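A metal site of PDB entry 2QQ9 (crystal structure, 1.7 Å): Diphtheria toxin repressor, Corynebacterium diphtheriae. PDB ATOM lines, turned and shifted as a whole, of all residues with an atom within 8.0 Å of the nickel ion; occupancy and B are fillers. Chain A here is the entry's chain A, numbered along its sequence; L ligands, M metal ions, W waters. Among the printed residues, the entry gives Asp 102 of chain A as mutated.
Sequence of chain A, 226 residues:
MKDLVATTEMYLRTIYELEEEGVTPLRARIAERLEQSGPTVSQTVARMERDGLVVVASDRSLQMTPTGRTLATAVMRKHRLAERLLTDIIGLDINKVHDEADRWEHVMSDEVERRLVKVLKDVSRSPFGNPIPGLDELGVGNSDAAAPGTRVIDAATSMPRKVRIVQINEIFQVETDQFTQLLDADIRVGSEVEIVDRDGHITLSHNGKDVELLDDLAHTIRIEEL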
ATOM      1  N   ARG A  13     -11.635  18.798  15.782  1.00  0.00           N
ATOM      2  CA  ARG A  13     -12.107  18.579  17.160  1.00  0.00           C
ATOM      3  C   ARG A  13     -11.076  17.702  17.883  1.00  0.00           C
ATOM      4  O   ARG A  13     -10.771  17.882  19.077  1.00  0.00           O
ATOM      5  CB  ARG A  13     -13.490  17.895  17.148  1.00  0.00           C
ATOM      6  CG  ARG A  13     -14.226  18.221  18.417  1.00  0.00           C
ATOM      7  CD  ARG A  13     -14.699  17.041  19.171  1.00  0.00           C
ATOM      8  NE  ARG A  13     -15.431  15.972  18.451  1.00  0.00           N
ATOM      9  CZ  ARG A  13     -15.366  14.687  18.757  1.00  0.00           C
ATOM     10  NH1 ARG A  13     -14.519  14.207  19.708  1.00  0.00           N
ATOM     11  NH2 ARG A  13     -16.072  13.804  18.033  1.00  0.00           N
ATOM     12  N   GLU A  17      -9.202  18.525  21.269  1.00  0.00           N
ATOM     13  CA  GLU A  17      -9.259  17.545  22.347  1.00  0.00           C
ATOM     14  C   GLU A  17      -7.890  17.226  22.944  1.00  0.00           C
ATOM     15  O   GLU A  17      -7.696  17.193  24.172  1.00  0.00           O
ATOM     16  CB  GLU A  17      -9.812  16.228  21.769  1.00  0.00           C
ATOM     17  CG  GLU A  17     -11.243  16.194  21.528  1.00  0.00           C
ATOM     18  CD  GLU A  17     -11.737  14.778  21.444  1.00  0.00           C
ATOM     19  OE1 GLU A  17     -10.957  13.839  21.077  1.00  0.00           O
ATOM     20  OE2 GLU A  17     -12.872  14.610  21.811  1.00  0.00           O
ATOM     21  N   MET A  76     -16.541  21.493  18.632  1.00  0.00           N
ATOM     22  CA  MET A  76     -16.545  21.037  20.060  1.00  0.00           C
ATOM     23  C   MET A  76     -17.844  21.511  20.784  1.00  0.00           C
ATOM     24  O   MET A  76     -18.456  20.766  21.505  1.00  0.00           O
ATOM     25  CB  MET A  76     -15.319  21.532  20.835  1.00  0.00           C
ATOM     26  CG  MET A  76     -15.216  20.929  22.234  1.00  0.00           C
ATOM     27  SD  MET A  76     -15.328  19.119  22.302  1.00  0.00           S
ATOM     28  CE  MET A  76     -13.578  18.612  22.162  1.00  0.00           C
ATOM     29  N   HIS A  79     -20.825  19.615  19.590  1.00  0.00           N
ATOM     30  CA  HIS A  79     -20.673  18.257  20.083  1.00  0.00           C
ATOM     31  C   HIS A  79     -21.170  18.205  21.528  1.00  0.00           C
ATOM     32  O   HIS A  79     -22.042  17.443  21.857  1.00  0.00           O
ATOM     33  CB  HIS A  79     -19.210  17.805  20.033  1.00  0.00           C
ATOM     34  CG  HIS A  79     -19.045  16.401  20.494  1.00  0.00           C
ATOM     35  ND1 HIS A  79     -19.484  15.313  19.771  1.00  0.00           N
ATOM     36  CD2 HIS A  79     -18.475  15.904  21.634  1.00  0.00           C
ATOM     37  CE1 HIS A  79     -19.174  14.198  20.431  1.00  0.00           C
ATOM     38  NE2 HIS A  79     -18.588  14.535  21.568  1.00  0.00           N
ATOM     39  N   ARG A  80     -20.581  19.037  22.363  1.00  0.00           N
ATOM     40  CA  ARG A  80     -20.973  19.065  23.773  1.00  0.00           C
ATOM     41  C   ARG A  80     -22.425  19.472  24.061  1.00  0.00           C
ATOM     42  O   ARG A  80     -23.076  18.877  24.955  1.00  0.00           O
ATOM     43  CB  ARG A  80     -19.955  19.860  24.598  1.00  0.00           C
ATOM     44  CG  ARG A  80     -18.618  19.284  24.499  1.00  0.00           C
ATOM     45  CD  ARG A  80     -17.580  19.893  25.484  1.00  0.00           C
ATOM     46  NE  ARG A  80     -16.466  18.963  25.571  1.00  0.00           N
ATOM     47  CZ  ARG A  80     -15.177  19.310  25.619  1.00  0.00           C
ATOM     48  NH1 ARG A  80     -14.817  20.577  25.663  1.00  0.00           N
ATOM     49  NH2 ARG A  80     -14.247  18.359  25.600  1.00  0.00           N
ATOM     50  N   GLU A  83     -24.517  16.466  23.222  1.00  0.00           N
ATOM     51  CA  GLU A  83     -24.407  15.519  24.331  1.00  0.00           C
ATOM     52  C   GLU A  83     -25.339  15.922  25.462  1.00  0.00           C
ATOM     53  O   GLU A  83     -26.128  15.090  25.929  1.00  0.00           O
ATOM     54  CB  GLU A  83     -22.964  15.422  24.794  1.00  0.00           C
ATOM     55  CG  GLU A  83     -22.108  14.669  23.774  1.00  0.00           C
ATOM     56  CD  GLU A  83     -20.654  14.496  24.182  1.00  0.00           C
ATOM     57  OE1 GLU A  83     -20.118  15.348  24.936  1.00  0.00           O
ATOM     58  OE2 GLU A  83     -20.104  13.437  23.830  1.00  0.00           O
ATOM     59  N   VAL A  97     -24.343   8.244  24.141  1.00  0.00           N
ATOM     60  CA  VAL A  97     -24.451   9.684  23.936  1.00  0.00           C
ATOM     61  C   VAL A  97     -23.317  10.257  23.092  1.00  0.00           C
ATOM     62  O   VAL A  97     -23.578  10.968  22.071  1.00  0.00           O
ATOM     63  CB  VAL A  97     -24.592  10.413  25.282  1.00  0.00           C
ATOM     64  CG1 VAL A  97     -24.354  11.880  25.140  1.00  0.00           C
ATOM     65  CG2 VAL A  97     -26.024  10.134  25.820  1.00  0.00           C
ATOM     66  N   HIS A  98     -22.089   9.905  23.484  1.00  0.00           N
ATOM     67  CA  HIS A  98     -20.927  10.384  22.704  1.00  0.00           C
ATOM     68  C   HIS A  98     -21.009  10.040  21.194  1.00  0.00           C
ATOM     69  O   HIS A  98     -20.838  10.898  20.347  1.00  0.00           O
ATOM     70  CB  HIS A  98     -19.548  10.005  23.298  1.00  0.00           C
ATOM     71  CG  HIS A  98     -18.451  10.314  22.343  1.00  0.00           C
ATOM     72  ND1 HIS A  98     -18.024  11.598  22.121  1.00  0.00           N
ATOM     73  CD2 HIS A  98     -17.833   9.538  21.413  1.00  0.00           C
ATOM     74  CE1 HIS A  98     -17.156  11.619  21.135  1.00  0.00           C
ATOM     75  NE2 HIS A  98     -17.017  10.382  20.669  1.00  0.00           N
ATOM     76  N   ASP A  99     -21.337   8.784  20.886  1.00  0.00           N
ATOM     77  CA  ASP A  99     -21.278   8.296  19.521  1.00  0.00           C
ATOM     78  C   ASP A  99     -22.339   9.027  18.731  1.00  0.00           C
ATOM     79  O   ASP A  99     -22.118   9.483  17.597  1.00  0.00           O
ATOM     80  CB  ASP A  99     -21.508   6.762  19.513  1.00  0.00           C
ATOM     81  CG  ASP A  99     -20.213   5.931  19.766  1.00  0.00           C
ATOM     82  OD1 ASP A  99     -19.082   6.470  19.748  1.00  0.00           O
ATOM     83  OD2 ASP A  99     -20.330   4.686  19.930  1.00  0.00           O
ATOM     84  N   GLU A 100     -23.490   9.203  19.362  1.00  0.00           N
ATOM     85  CA  GLU A 100     -24.551   9.933  18.667  1.00  0.00           C
ATOM     86  C   GLU A 100     -24.128  11.377  18.367  1.00  0.00           C
ATOM     87  O   GLU A 100     -24.220  11.835  17.220  1.00  0.00           O
ATOM     88  CB  GLU A 100     -25.866   9.900  19.470  1.00  0.00           C
ATOM     89  CG  GLU A 100     -27.050  10.375  18.658  1.00  0.00           C
ATOM     90  CD  GLU A 100     -27.746   9.256  17.929  1.00  0.00           C
ATOM     91  OE1 GLU A 100     -27.560   8.094  18.365  1.00  0.00           O
ATOM     92  OE2 GLU A 100     -28.490   9.561  16.986  1.00  0.00           O
ATOM     93  N   ALA A 101     -23.536  12.025  19.389  1.00  0.00           N
ATOM     94  CA  ALA A 101     -23.083  13.419  19.242  1.00  0.00           C
ATOM     95  C   ALA A 101     -21.926  13.539  18.255  1.00  0.00           C
ATOM     96  O   ALA A 101     -21.712  14.634  17.678  1.00  0.00           O
ATOM     97  CB  ALA A 101     -22.712  13.986  20.533  1.00  0.00           C
ATOM     98  N   ASP A 102     -21.228  12.436  18.061  1.00  0.00           N
ATOM     99  CA  ASP A 102     -20.105  12.338  17.146  1.00  0.00           C
ATOM    100  C   ASP A 102     -20.683  12.559  15.743  1.00  0.00           C
ATOM    101  O   ASP A 102     -20.068  13.192  14.866  1.00  0.00           O
ATOM    102  CB  ASP A 102     -19.379  10.968  17.279  1.00  0.00           C
ATOM    103  CG  ASP A 102     -17.977  10.916  16.576  1.00  0.00           C
ATOM    104  OD1 ASP A 102     -17.485  11.939  16.028  1.00  0.00           O
ATOM    105  OD2 ASP A 102     -17.370   9.861  16.670  1.00  0.00           O
ATOM    106  N   GLU A 105     -22.829  16.540  15.804  1.00  0.00           N
ATOM    107  CA  GLU A 105     -21.912  17.686  15.796  1.00  0.00           C
ATOM    108  C   GLU A 105     -21.625  18.313  14.376  1.00  0.00           C
ATOM    109  O   GLU A 105     -21.327  19.528  14.275  1.00  0.00           O
ATOM    110  CB  GLU A 105     -20.614  17.333  16.521  1.00  0.00           C
ATOM    111  CG  GLU A 105     -19.722  16.310  15.701  1.00  0.00           C
ATOM    112  CD  GLU A 105     -18.442  15.949  16.437  1.00  0.00           C
ATOM    113  OE1 GLU A 105     -17.936  16.736  17.271  1.00  0.00           O
ATOM    114  OE2 GLU A 105     -17.944  14.889  16.187  1.00  0.00           O
ATOM    115  N   SER A 126     -20.142  19.530  29.356  1.00  0.00           N
ATOM    116  CA  SER A 126     -20.744  18.315  28.762  1.00  0.00           C
ATOM    117  C   SER A 126     -21.104  17.386  29.899  1.00  0.00           C
ATOM    118  O   SER A 126     -20.679  17.581  31.032  1.00  0.00           O
ATOM    119  CB  SER A 126     -19.761  17.590  27.855  1.00  0.00           C
ATOM    120  OG  SER A 126     -18.775  16.916  28.636  1.00  0.00           O
ATOM    121  N   PRO A 127     -21.847  16.319  29.577  1.00  0.00           N
ATOM    122  CA  PRO A 127     -22.116  15.289  30.608  1.00  0.00           C
ATOM    123  C   PRO A 127     -20.838  14.515  31.048  1.00  0.00           C
ATOM    124  O   PRO A 127     -20.892  13.758  32.004  1.00  0.00           O
ATOM    125  CB  PRO A 127     -23.151  14.362  29.918  1.00  0.00           C
ATOM    126  CG  PRO A 127     -23.587  15.194  28.549  1.00  0.00           C
ATOM    127  CD  PRO A 127     -22.404  16.018  28.242  1.00  0.00           C
ATOM    128  N   PHE A 128     -19.733  14.715  30.309  1.00  0.00           N
ATOM    129  CA  PHE A 128     -18.471  13.991  30.557  1.00  0.00           C
ATOM    130  C   PHE A 128     -17.400  14.859  31.223  1.00  0.00           C
ATOM    131  O   PHE A 128     -16.191  14.508  31.262  1.00  0.00           O
ATOM    132  CB  PHE A 128     -17.990  13.423  29.234  1.00  0.00           C
ATOM    133  CG  PHE A 128     -19.044  12.554  28.542  1.00  0.00           C
ATOM    134  CD1 PHE A 128     -19.382  11.354  29.100  1.00  0.00           C
ATOM    135  CD2 PHE A 128     -19.768  13.006  27.435  1.00  0.00           C
ATOM    136  CE1 PHE A 128     -20.349  10.540  28.532  1.00  0.00           C
ATOM    137  CE2 PHE A 128     -20.729  12.194  26.859  1.00  0.00           C
ATOM    138  CZ  PHE A 128     -21.037  10.963  27.423  1.00  0.00           C
ATOM    139  N   ASN A 130     -16.431  18.179  30.801  1.00  0.00           N
ATOM    140  CA  ASN A 130     -15.568  19.145  30.111  1.00  0.00           C
ATOM    141  C   ASN A 130     -16.273  20.448  29.790  1.00  0.00           C
ATOM    142  O   ASN A 130     -17.405  20.414  29.317  1.00  0.00           O
ATOM    143  CB  ASN A 130     -15.063  18.485  28.818  1.00  0.00           C
ATOM    144  CG  ASN A 130     -14.324  17.208  29.130  1.00  0.00           C
ATOM    145  OD1 ASN A 130     -13.433  17.203  29.994  1.00  0.00           O
ATOM    146  ND2 ASN A 130     -14.675  16.116  28.465  1.00  0.00           N
HETATM  147  P1  LIG L   1     -16.564  15.232  25.630  1.00  0.00           P
HETATM  148  O1  LIG L   1     -17.705  15.130  24.597  1.00  0.00           O
HETATM  149  O2  LIG L   1     -16.942  16.368  26.574  1.00  0.00           O
HETATM  150  O3  LIG L   1     -15.313  15.714  24.863  1.00  0.00           O
HETATM  151  O4  LIG L   1     -16.395  13.945  26.405  1.00  0.00           O
HETATM  152 NI    NI M   1     -17.986  13.377  23.328  1.00  0.00          NI
HETATM  153  O   HOH W   1     -17.528  12.010  25.058  1.00  0.00           O
HETATM  154  O   HOH W   2     -15.813  13.689  23.006  1.00  0.00           O
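Of the 17 residues printed, 3 come within 4 Å of the nickel ion.
The nearest printed residue that does not touch the nickel ion is Phe 128 (4.5 Å).
O of Ala 101 is in hydrogen-bond range of ND1 of His 79 (3.1 Å).
A ring nitrogen (ND1) of His 79 sits close to the side-chain carboxylate (OE1) of Glu 105, 3.3 Å away.
ND1 of His 98 binds the nickel ion (2.2 Å).
The nickel ion is bound by OE2 of Glu 83, at 2.2 Å.
O1 of the ligand is bound to the nickel ion (2.2 Å).
NE2 of His 79 is bound to the nickel ion (2.2 Å).
The nickel ion is bound by water W2.
Water W1 binds the nickel ion (2.3 Å).
The nickel ion has six donor atoms within binding distance.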
